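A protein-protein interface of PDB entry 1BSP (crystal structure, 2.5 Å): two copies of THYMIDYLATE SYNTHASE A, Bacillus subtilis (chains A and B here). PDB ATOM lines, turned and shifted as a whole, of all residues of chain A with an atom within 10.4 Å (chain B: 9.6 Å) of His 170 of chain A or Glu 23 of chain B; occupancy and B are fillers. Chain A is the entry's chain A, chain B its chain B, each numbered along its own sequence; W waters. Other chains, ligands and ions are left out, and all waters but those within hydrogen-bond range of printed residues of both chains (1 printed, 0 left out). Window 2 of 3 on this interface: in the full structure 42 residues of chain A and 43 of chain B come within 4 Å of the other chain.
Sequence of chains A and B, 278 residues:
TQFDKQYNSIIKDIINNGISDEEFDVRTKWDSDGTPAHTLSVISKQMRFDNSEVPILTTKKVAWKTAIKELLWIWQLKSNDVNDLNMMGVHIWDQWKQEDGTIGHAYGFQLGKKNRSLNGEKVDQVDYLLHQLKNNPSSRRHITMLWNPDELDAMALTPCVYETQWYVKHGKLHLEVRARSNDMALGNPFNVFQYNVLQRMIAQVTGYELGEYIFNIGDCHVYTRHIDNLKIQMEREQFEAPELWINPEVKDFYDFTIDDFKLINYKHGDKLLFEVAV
The side-chain amino group of Lys 169 of chain A sits at hydrogen-bond distance from the side-chain hydroxyl of Ser 41 of chain B, at 2.8 Å.
Of the 16 printed residues of chain A, 6 touch a printed residue of chain B.
Hydrophobic or aromatic side chains of chain A within 4 Å of the printed part of chain B: Pro 137, Tyr 167, His 170 and His 174.
Of the 15 printed residues of chain B, 5 touch a printed residue of chain A.
Among the printed residues, no Asp or Glu carboxylate lies within 4 Å of a Lys or Arg side-chain nitrogen of the other chain.
Water W1 lies within hydrogen-bond range of N of His 170 of chain A, O of Ser 20 of chain B and OE2 of Glu 23 of chain B.
Among the printed residues, pairs that only touch across the chains: His 170 of chain A with Glu 23 of chain B (3.5 Å), Pro 137 of chain A with Phe 24 of chain B (3.5 Å), His 174 of chain A with Ile 43 of chain B (3.6 Å), Tyr 167 of chain A with Ile 43 of chain B (3.7 Å), Lys 169 of chain A with Ile 43 of chain B (3.8 Å), Ser 138 of chain A with Phe 24 of chain B (3.9 Å) and Ser 138 of chain A with Asp 25 of chain B (3.95 Å).
The backbone carbonyl oxygen (O) of Tyr 167 of chain A lies within hydrogen-bond range of the backbone NH (N) of His 174 of chain A (2.8 Å).
A ring nitrogen (ND1) of His 174 of chain A lies within hydrogen-bond range of the backbone NH (N) of Glu 212 of chain A (3.1 Å).
The backbone NH (N) of Ile 19 of chain B sits at hydrogen-bond distance from the backbone carbonyl oxygen (O) of Ser 41 of chain B (3.0 Å).
Printed residues of chain B within 4 Å of His 170 of chain A: Glu 23 (3.5 Å).
No residue of chain B comes within 4 Å of Gly 171 of chain A.
Of the printed residues of chain B, Ser 138 of chain A touches Phe 24 and Asp 25.
Printed residues of chain A within 4 Å of Asp 25 of chain B: Ser 138.
Of the printed residues of chain B, His 174 of chain A touches Ile 43.
The nearest residue of chain B that does not touch His 170 of chain A is Ile 19 of chain B (4.1 Å).
No position is printed for both chains.
Of the 8 pairs that touch across the chains among the printed residues, none has its exchanged pair printed and touching as well.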
ATOM      1  N   PRO A 137      -1.390 -24.707  -2.897  1.00  0.00           N
ATOM      2  CA  PRO A 137      -0.423 -23.829  -3.551  1.00  0.00           C
ATOM      3  C   PRO A 137      -0.982 -22.945  -4.675  1.00  0.00           C
ATOM      4  O   PRO A 137      -0.752 -21.736  -4.687  1.00  0.00           O
ATOM      5  CB  PRO A 137       0.631 -24.820  -4.055  1.00  0.00           C
ATOM      6  CG  PRO A 137      -0.174 -26.025  -4.345  1.00  0.00           C
ATOM      7  CD  PRO A 137      -1.042 -26.115  -3.125  1.00  0.00           C
ATOM      8  N   SER A 138      -1.781 -23.534  -5.557  1.00  0.00           N
ATOM      9  CA  SER A 138      -2.359 -22.829  -6.705  1.00  0.00           C
ATOM     10  C   SER A 138      -3.220 -21.608  -6.384  1.00  0.00           C
ATOM     11  O   SER A 138      -3.626 -20.887  -7.298  1.00  0.00           O
ATOM     12  CB  SER A 138      -3.188 -23.804  -7.538  1.00  0.00           C
ATOM     13  OG  SER A 138      -4.228 -24.352  -6.743  1.00  0.00           O
ATOM     14  N   TYR A 167       3.141 -16.570  -4.019  1.00  0.00           N
ATOM     15  CA  TYR A 167       2.718 -17.352  -5.173  1.00  0.00           C
ATOM     16  C   TYR A 167       3.585 -18.590  -5.311  1.00  0.00           C
ATOM     17  O   TYR A 167       4.812 -18.496  -5.238  1.00  0.00           O
ATOM     18  CB  TYR A 167       2.887 -16.567  -6.483  1.00  0.00           C
ATOM     19  CG  TYR A 167       2.451 -15.117  -6.474  1.00  0.00           C
ATOM     20  CD1 TYR A 167       3.298 -14.116  -5.975  1.00  0.00           C
ATOM     21  CD2 TYR A 167       1.219 -14.737  -7.014  1.00  0.00           C
ATOM     22  CE1 TYR A 167       2.933 -12.784  -6.019  1.00  0.00           C
ATOM     23  CE2 TYR A 167       0.844 -13.416  -7.066  1.00  0.00           C
ATOM     24  CZ  TYR A 167       1.702 -12.438  -6.569  1.00  0.00           C
ATOM     25  OH  TYR A 167       1.325 -11.118  -6.636  1.00  0.00           O
ATOM     26  N   VAL A 168       2.958 -19.743  -5.515  1.00  0.00           N
ATOM     27  CA  VAL A 168       3.709 -20.973  -5.751  1.00  0.00           C
ATOM     28  C   VAL A 168       3.570 -21.220  -7.255  1.00  0.00           C
ATOM     29  O   VAL A 168       2.473 -21.477  -7.735  1.00  0.00           O
ATOM     30  CB  VAL A 168       3.144 -22.173  -4.971  1.00  0.00           C
ATOM     31  CG1 VAL A 168       3.984 -23.374  -5.234  1.00  0.00           C
ATOM     32  CG2 VAL A 168       3.129 -21.880  -3.473  1.00  0.00           C
ATOM     33  N   LYS A 169       4.653 -21.029  -8.006  1.00  0.00           N
ATOM     34  CA  LYS A 169       4.629 -21.239  -9.457  1.00  0.00           C
ATOM     35  C   LYS A 169       5.784 -22.148  -9.839  1.00  0.00           C
ATOM     36  O   LYS A 169       6.934 -21.703  -9.882  1.00  0.00           O
ATOM     37  CB  LYS A 169       4.793 -19.925 -10.231  1.00  0.00           C
ATOM     38  CG  LYS A 169       3.779 -18.839  -9.936  1.00  0.00           C
ATOM     39  CD  LYS A 169       2.383 -19.203 -10.416  1.00  0.00           C
ATOM     40  CE  LYS A 169       1.442 -17.998 -10.348  1.00  0.00           C
ATOM     41  NZ  LYS A 169       0.093 -18.290 -10.916  1.00  0.00           N
ATOM     42  N   HIS A 170       5.478 -23.408 -10.131  1.00  0.00           N
ATOM     43  CA  HIS A 170       6.476 -24.409 -10.516  1.00  0.00           C
ATOM     44  C   HIS A 170       7.419 -24.821  -9.381  1.00  0.00           C
ATOM     45  O   HIS A 170       8.637 -24.871  -9.559  1.00  0.00           O
ATOM     46  CB  HIS A 170       7.290 -23.942 -11.737  1.00  0.00           C
ATOM     47  CG  HIS A 170       7.277 -24.914 -12.881  1.00  0.00           C
ATOM     48  ND1 HIS A 170       8.419 -25.296 -13.556  1.00  0.00           N
ATOM     49  CD2 HIS A 170       6.267 -25.644 -13.415  1.00  0.00           C
ATOM     50  CE1 HIS A 170       8.116 -26.221 -14.448  1.00  0.00           C
ATOM     51  NE2 HIS A 170       6.818 -26.452 -14.380  1.00  0.00           N
ATOM     52  N   GLY A 171       6.848 -25.141  -8.224  1.00  0.00           N
ATOM     53  CA  GLY A 171       7.653 -25.554  -7.087  1.00  0.00           C
ATOM     54  C   GLY A 171       8.421 -24.447  -6.387  1.00  0.00           C
ATOM     55  O   GLY A 171       9.046 -24.684  -5.346  1.00  0.00           O
ATOM     56  N   LYS A 172       8.324 -23.233  -6.928  1.00  0.00           N
ATOM     57  CA  LYS A 172       8.999 -22.046  -6.400  1.00  0.00           C
ATOM     58  C   LYS A 172       8.076 -21.137  -5.618  1.00  0.00           C
ATOM     59  O   LYS A 172       6.948 -20.920  -6.029  1.00  0.00           O
ATOM     60  CB  LYS A 172       9.567 -21.248  -7.557  1.00  0.00           C
ATOM     61  CG  LYS A 172      11.045 -21.195  -7.591  1.00  0.00           C
ATOM     62  CD  LYS A 172      11.546 -21.607  -8.937  1.00  0.00           C
ATOM     63  CE  LYS A 172      12.834 -20.901  -9.239  1.00  0.00           C
ATOM     64  NZ  LYS A 172      13.720 -21.715 -10.108  1.00  0.00           N
ATOM     65  N   LEU A 173       8.574 -20.571  -4.524  1.00  0.00           N
ATOM     66  CA  LEU A 173       7.788 -19.653  -3.702  1.00  0.00           C
ATOM     67  C   LEU A 173       8.234 -18.212  -3.967  1.00  0.00           C
ATOM     68  O   LEU A 173       9.392 -17.855  -3.705  1.00  0.00           O
ATOM     69  CB  LEU A 173       7.948 -19.975  -2.219  1.00  0.00           C
ATOM     70  CG  LEU A 173       6.944 -19.275  -1.309  1.00  0.00           C
ATOM     71  CD1 LEU A 173       5.553 -19.496  -1.827  1.00  0.00           C
ATOM     72  CD2 LEU A 173       7.057 -19.788   0.106  1.00  0.00           C
ATOM     73  N   HIS A 174       7.323 -17.413  -4.528  1.00  0.00           N
ATOM     74  CA  HIS A 174       7.559 -16.001  -4.864  1.00  0.00           C
ATOM     75  C   HIS A 174       6.894 -15.118  -3.828  1.00  0.00           C
ATOM     76  O   HIS A 174       5.823 -15.466  -3.302  1.00  0.00           O
ATOM     77  CB  HIS A 174       6.962 -15.667  -6.230  1.00  0.00           C
ATOM     78  CG  HIS A 174       7.274 -16.679  -7.284  1.00  0.00           C
ATOM     79  ND1 HIS A 174       8.242 -16.478  -8.244  1.00  0.00           N
ATOM     80  CD2 HIS A 174       6.774 -17.918  -7.503  1.00  0.00           C
ATOM     81  CE1 HIS A 174       8.331 -17.554  -9.006  1.00  0.00           C
ATOM     82  NE2 HIS A 174       7.450 -18.442  -8.578  1.00  0.00           N
ATOM     83  N   GLY A 207       8.952 -26.169   2.253  1.00  0.00           N
ATOM     84  CA  GLY A 207       9.611 -27.032   1.293  1.00  0.00           C
ATOM     85  C   GLY A 207       9.512 -26.599  -0.154  1.00  0.00           C
ATOM     86  O   GLY A 207       9.278 -27.416  -1.044  1.00  0.00           O
ATOM     87  N   TYR A 208       9.703 -25.317  -0.405  1.00  0.00           N
ATOM     88  CA  TYR A 208       9.652 -24.807  -1.759  1.00  0.00           C
ATOM     89  C   TYR A 208      10.994 -24.193  -2.071  1.00  0.00           C
ATOM     90  O   TYR A 208      11.718 -23.784  -1.167  1.00  0.00           O
ATOM     91  CB  TYR A 208       8.579 -23.733  -1.894  1.00  0.00           C
ATOM     92  CG  TYR A 208       7.194 -24.290  -1.902  1.00  0.00           C
ATOM     93  CD1 TYR A 208       6.759 -25.093  -2.953  1.00  0.00           C
ATOM     94  CD2 TYR A 208       6.315 -24.041  -0.849  1.00  0.00           C
ATOM     95  CE1 TYR A 208       5.480 -25.637  -2.955  1.00  0.00           C
ATOM     96  CE2 TYR A 208       5.028 -24.583  -0.842  1.00  0.00           C
ATOM     97  CZ  TYR A 208       4.625 -25.381  -1.899  1.00  0.00           C
ATOM     98  OH  TYR A 208       3.382 -25.953  -1.906  1.00  0.00           O
ATOM     99  N   GLU A 209      11.344 -24.159  -3.345  1.00  0.00           N
ATOM    100  CA  GLU A 209      12.589 -23.547  -3.743  1.00  0.00           C
ATOM    101  C   GLU A 209      12.301 -22.038  -3.723  1.00  0.00           C
ATOM    102  O   GLU A 209      11.136 -21.630  -3.628  1.00  0.00           O
ATOM    103  CB  GLU A 209      12.989 -24.040  -5.136  1.00  0.00           C
ATOM    104  CG  GLU A 209      14.376 -23.635  -5.562  1.00  0.00           C
ATOM    105  CD  GLU A 209      14.803 -24.290  -6.856  1.00  0.00           C
ATOM    106  OE1 GLU A 209      14.209 -23.991  -7.916  1.00  0.00           O
ATOM    107  OE2 GLU A 209      15.749 -25.101  -6.817  1.00  0.00           O
ATOM    108  N   LEU A 210      13.342 -21.212  -3.776  1.00  0.00           N
ATOM    109  CA  LEU A 210      13.158 -19.769  -3.745  1.00  0.00           C
ATOM    110  C   LEU A 210      12.762 -19.171  -5.083  1.00  0.00           C
ATOM    111  O   LEU A 210      13.427 -19.392  -6.098  1.00  0.00           O
ATOM    112  CB  LEU A 210      14.412 -19.074  -3.220  1.00  0.00           C
ATOM    113  CG  LEU A 210      14.623 -19.178  -1.707  1.00  0.00           C
ATOM    114  CD1 LEU A 210      15.927 -18.503  -1.278  1.00  0.00           C
ATOM    115  CD2 LEU A 210      13.418 -18.564  -1.010  1.00  0.00           C
ATOM    116  N   GLY A 211      11.657 -18.430  -5.067  1.00  0.00           N
ATOM    117  CA  GLY A 211      11.173 -17.771  -6.256  1.00  0.00           C
ATOM    118  C   GLY A 211      11.651 -16.332  -6.261  1.00  0.00           C
ATOM    119  O   GLY A 211      12.628 -15.988  -5.593  1.00  0.00           O
ATOM    120  N   GLU A 212      10.915 -15.471  -6.952  1.00  0.00           N
ATOM    121  CA  GLU A 212      11.278 -14.061  -7.061  1.00  0.00           C
ATOM    122  C   GLU A 212      10.821 -13.224  -5.853  1.00  0.00           C
ATOM    123  O   GLU A 212       9.814 -13.543  -5.211  1.00  0.00           O
ATOM    124  CB  GLU A 212      10.715 -13.501  -8.372  1.00  0.00           C
ATOM    125  CG  GLU A 212      11.283 -12.159  -8.803  1.00  0.00           C
ATOM    126  CD  GLU A 212      10.798 -11.725 -10.183  1.00  0.00           C
ATOM    127  OE1 GLU A 212       9.709 -12.166 -10.611  1.00  0.00           O
ATOM    128  OE2 GLU A 212      11.513 -10.934 -10.846  1.00  0.00           O
ATOM    129  N   GLY B  18       4.983 -17.075 -19.719  1.00  0.00           N
ATOM    130  CA  GLY B  18       4.081 -17.523 -18.677  1.00  0.00           C
ATOM    131  C   GLY B  18       4.415 -18.874 -18.085  1.00  0.00           C
ATOM    132  O   GLY B  18       5.128 -19.683 -18.683  1.00  0.00           O
ATOM    133  N   ILE B  19       3.894 -19.105 -16.891  1.00  0.00           N
ATOM    134  CA  ILE B  19       4.072 -20.354 -16.176  1.00  0.00           C
ATOM    135  C   ILE B  19       2.664 -20.881 -15.929  1.00  0.00           C
ATOM    136  O   ILE B  19       1.835 -20.190 -15.331  1.00  0.00           O
ATOM    137  CB  ILE B  19       4.779 -20.138 -14.812  1.00  0.00           C
ATOM    138  CG1 ILE B  19       6.154 -19.516 -15.029  1.00  0.00           C
ATOM    139  CG2 ILE B  19       4.953 -21.470 -14.082  1.00  0.00           C
ATOM    140  CD1 ILE B  19       6.843 -19.111 -13.744  1.00  0.00           C
ATOM    141  N   SER B  20       2.386 -22.087 -16.411  1.00  0.00           N
ATOM    142  CA  SER B  20       1.071 -22.670 -16.241  1.00  0.00           C
ATOM    143  C   SER B  20       0.921 -23.278 -14.869  1.00  0.00           C
ATOM    144  O   SER B  20       1.895 -23.407 -14.130  1.00  0.00           O
ATOM    145  CB  SER B  20       0.827 -23.735 -17.315  1.00  0.00           C
ATOM    146  OG  SER B  20       1.873 -24.695 -17.370  1.00  0.00           O
ATOM    147  N   ASP B  21      -0.309 -23.629 -14.522  1.00  0.00           N
ATOM    148  CA  ASP B  21      -0.593 -24.269 -13.249  1.00  0.00           C
ATOM    149  C   ASP B  21      -1.228 -25.610 -13.613  1.00  0.00           C
ATOM    150  O   ASP B  21      -2.099 -26.115 -12.903  1.00  0.00           O
ATOM    151  CB  ASP B  21      -1.557 -23.420 -12.412  1.00  0.00           C
ATOM    152  CG  ASP B  21      -2.895 -23.174 -13.102  1.00  0.00           C
ATOM    153  OD1 ASP B  21      -3.058 -23.539 -14.280  1.00  0.00           O
ATOM    154  OD2 ASP B  21      -3.800 -22.599 -12.459  1.00  0.00           O
ATOM    155  N   GLU B  22      -0.802 -26.156 -14.751  1.00  0.00           N
ATOM    156  CA  GLU B  22      -1.326 -27.417 -15.275  1.00  0.00           C
ATOM    157  C   GLU B  22      -1.127 -28.651 -14.409  1.00  0.00           C
ATOM    158  O   GLU B  22      -1.934 -29.585 -14.480  1.00  0.00           O
ATOM    159  CB  GLU B  22      -0.819 -27.662 -16.700  1.00  0.00           C
ATOM    160  CG  GLU B  22      -1.678 -26.952 -17.765  1.00  0.00           C
ATOM    161  CD  GLU B  22      -0.938 -26.645 -19.060  1.00  0.00           C
ATOM    162  OE1 GLU B  22       0.285 -26.390 -19.014  1.00  0.00           O
ATOM    163  OE2 GLU B  22      -1.596 -26.606 -20.123  1.00  0.00           O
ATOM    164  N   GLU B  23      -0.104 -28.632 -13.557  1.00  0.00           N
ATOM    165  CA  GLU B  23       0.179 -29.770 -12.693  1.00  0.00           C
ATOM    166  C   GLU B  23      -0.598 -29.740 -11.379  1.00  0.00           C
ATOM    167  O   GLU B  23      -0.522 -30.688 -10.599  1.00  0.00           O
ATOM    168  CB  GLU B  23       1.679 -29.860 -12.409  1.00  0.00           C
ATOM    169  CG  GLU B  23       2.199 -28.857 -11.386  1.00  0.00           C
ATOM    170  CD  GLU B  23       2.851 -27.637 -12.012  1.00  0.00           C
ATOM    171  OE1 GLU B  23       2.361 -27.145 -13.053  1.00  0.00           O
ATOM    172  OE2 GLU B  23       3.863 -27.161 -11.453  1.00  0.00           O
ATOM    173  N   PHE B  24      -1.347 -28.663 -11.143  1.00  0.00           N
ATOM    174  CA  PHE B  24      -2.116 -28.512  -9.910  1.00  0.00           C
ATOM    175  C   PHE B  24      -3.588 -28.811 -10.088  1.00  0.00           C
ATOM    176  O   PHE B  24      -4.128 -28.689 -11.189  1.00  0.00           O
ATOM    177  CB  PHE B  24      -2.020 -27.081  -9.381  1.00  0.00           C
ATOM    178  CG  PHE B  24      -0.649 -26.671  -8.946  1.00  0.00           C
ATOM    179  CD1 PHE B  24      -0.042 -27.283  -7.857  1.00  0.00           C
ATOM    180  CD2 PHE B  24       0.028 -25.650  -9.606  1.00  0.00           C
ATOM    181  CE1 PHE B  24       1.219 -26.886  -7.434  1.00  0.00           C
ATOM    182  CE2 PHE B  24       1.293 -25.244  -9.190  1.00  0.00           C
ATOM    183  CZ  PHE B  24       1.891 -25.863  -8.099  1.00  0.00           C
ATOM    184  N   ASP B  25      -4.246 -29.142  -8.978  1.00  0.00           N
ATOM    185  CA  ASP B  25      -5.684 -29.393  -8.968  1.00  0.00           C
ATOM    186  C   ASP B  25      -6.314 -28.023  -8.744  1.00  0.00           C
ATOM    187  O   ASP B  25      -6.385 -27.546  -7.611  1.00  0.00           O
ATOM    188  CB  ASP B  25      -6.073 -30.322  -7.817  1.00  0.00           C
ATOM    189  CG  ASP B  25      -5.747 -31.767  -8.099  1.00  0.00           C
ATOM    190  OD1 ASP B  25      -6.407 -32.355  -8.983  1.00  0.00           O
ATOM    191  OD2 ASP B  25      -4.834 -32.314  -7.439  1.00  0.00           O
ATOM    192  N   VAL B  26      -6.748 -27.387  -9.828  1.00  0.00           N
ATOM    193  CA  VAL B  26      -7.343 -26.054  -9.773  1.00  0.00           C
ATOM    194  C   VAL B  26      -8.838 -26.021  -9.458  1.00  0.00           C
ATOM    195  O   VAL B  26      -9.592 -26.901  -9.880  1.00  0.00           O
ATOM    196  CB  VAL B  26      -7.083 -25.293 -11.087  1.00  0.00           C
ATOM    197  CG1 VAL B  26      -5.591 -25.101 -11.278  1.00  0.00           C
ATOM    198  CG2 VAL B  26      -7.671 -26.053 -12.271  1.00  0.00           C
ATOM    199  N   PRO B  36     -10.950 -28.953 -15.840  1.00  0.00           N
ATOM    200  CA  PRO B  36     -10.200 -27.929 -15.105  1.00  0.00           C
ATOM    201  C   PRO B  36      -9.730 -26.790 -15.993  1.00  0.00           C
ATOM    202  O   PRO B  36      -9.120 -27.019 -17.038  1.00  0.00           O
ATOM    203  CB  PRO B  36      -9.020 -28.717 -14.531  1.00  0.00           C
ATOM    204  CG  PRO B  36      -8.848 -29.855 -15.516  1.00  0.00           C
ATOM    205  CD  PRO B  36     -10.275 -30.259 -15.755  1.00  0.00           C
ATOM    206  N   HIS B  38      -7.277 -24.128 -16.647  1.00  0.00           N
ATOM    207  CA  HIS B  38      -5.920 -23.749 -16.304  1.00  0.00           C
ATOM    208  C   HIS B  38      -5.521 -22.379 -16.820  1.00  0.00           C
ATOM    209  O   HIS B  38      -5.960 -21.934 -17.885  1.00  0.00           O
ATOM    210  CB  HIS B  38      -4.931 -24.821 -16.774  1.00  0.00           C
ATOM    211  CG  HIS B  38      -4.949 -26.056 -15.929  1.00  0.00           C
ATOM    212  ND1 HIS B  38      -4.555 -26.060 -14.608  1.00  0.00           N
ATOM    213  CD2 HIS B  38      -5.356 -27.316 -16.204  1.00  0.00           C
ATOM    214  CE1 HIS B  38      -4.721 -27.269 -14.102  1.00  0.00           C
ATOM    215  NE2 HIS B  38      -5.207 -28.050 -15.052  1.00  0.00           N
ATOM    216  N   THR B  39      -4.685 -21.708 -16.050  1.00  0.00           N
ATOM    217  CA  THR B  39      -4.214 -20.394 -16.420  1.00  0.00           C
ATOM    218  C   THR B  39      -2.735 -20.455 -16.761  1.00  0.00           C
ATOM    219  O   THR B  39      -2.072 -21.464 -16.526  1.00  0.00           O
ATOM    220  CB  THR B  39      -4.437 -19.427 -15.265  1.00  0.00           C
ATOM    221  OG1 THR B  39      -3.940 -20.016 -14.055  1.00  0.00           O
ATOM    222  CG2 THR B  39      -5.909 -19.148 -15.101  1.00  0.00           C
ATOM    223  N   LEU B  40      -2.250 -19.385 -17.366  1.00  0.00           N
ATOM    224  CA  LEU B  40      -0.858 -19.238 -17.762  1.00  0.00           C
ATOM    225  C   LEU B  40      -0.566 -17.843 -17.191  1.00  0.00           C
ATOM    226  O   LEU B  40      -1.307 -16.893 -17.476  1.00  0.00           O
ATOM    227  CB  LEU B  40      -0.800 -19.231 -19.280  1.00  0.00           C
ATOM    228  CG  LEU B  40       0.531 -19.397 -19.990  1.00  0.00           C
ATOM    229  CD1 LEU B  40       1.146 -20.716 -19.628  1.00  0.00           C
ATOM    230  CD2 LEU B  40       0.283 -19.323 -21.472  1.00  0.00           C
ATOM    231  N   SER B  41       0.448 -17.700 -16.345  1.00  0.00           N
ATOM    232  CA  SER B  41       0.663 -16.386 -15.759  1.00  0.00           C
ATOM    233  C   SER B  41       2.043 -15.806 -15.584  1.00  0.00           C
ATOM    234  O   SER B  41       3.054 -16.493 -15.679  1.00  0.00           O
ATOM    235  CB  SER B  41      -0.060 -16.307 -14.417  1.00  0.00           C
ATOM    236  OG  SER B  41       0.527 -17.164 -13.461  1.00  0.00           O
ATOM    237  N   ILE B  43       3.986 -12.748 -12.972  1.00  0.00           N
ATOM    238  CA  ILE B  43       3.821 -12.162 -11.644  1.00  0.00           C
ATOM    239  C   ILE B  43       4.237 -10.705 -11.585  1.00  0.00           C
ATOM    240  O   ILE B  43       5.303 -10.337 -12.069  1.00  0.00           O
ATOM    241  CB  ILE B  43       4.624 -12.952 -10.579  1.00  0.00           C
ATOM    242  CG1 ILE B  43       3.936 -14.281 -10.276  1.00  0.00           C
ATOM    243  CG2 ILE B  43       4.745 -12.163  -9.279  1.00  0.00           C
ATOM    244  CD1 ILE B  43       4.759 -15.179  -9.366  1.00  0.00           C
HETATM  245  O   HOH W   1       3.002 -24.065 -11.517  1.00  0.00           O
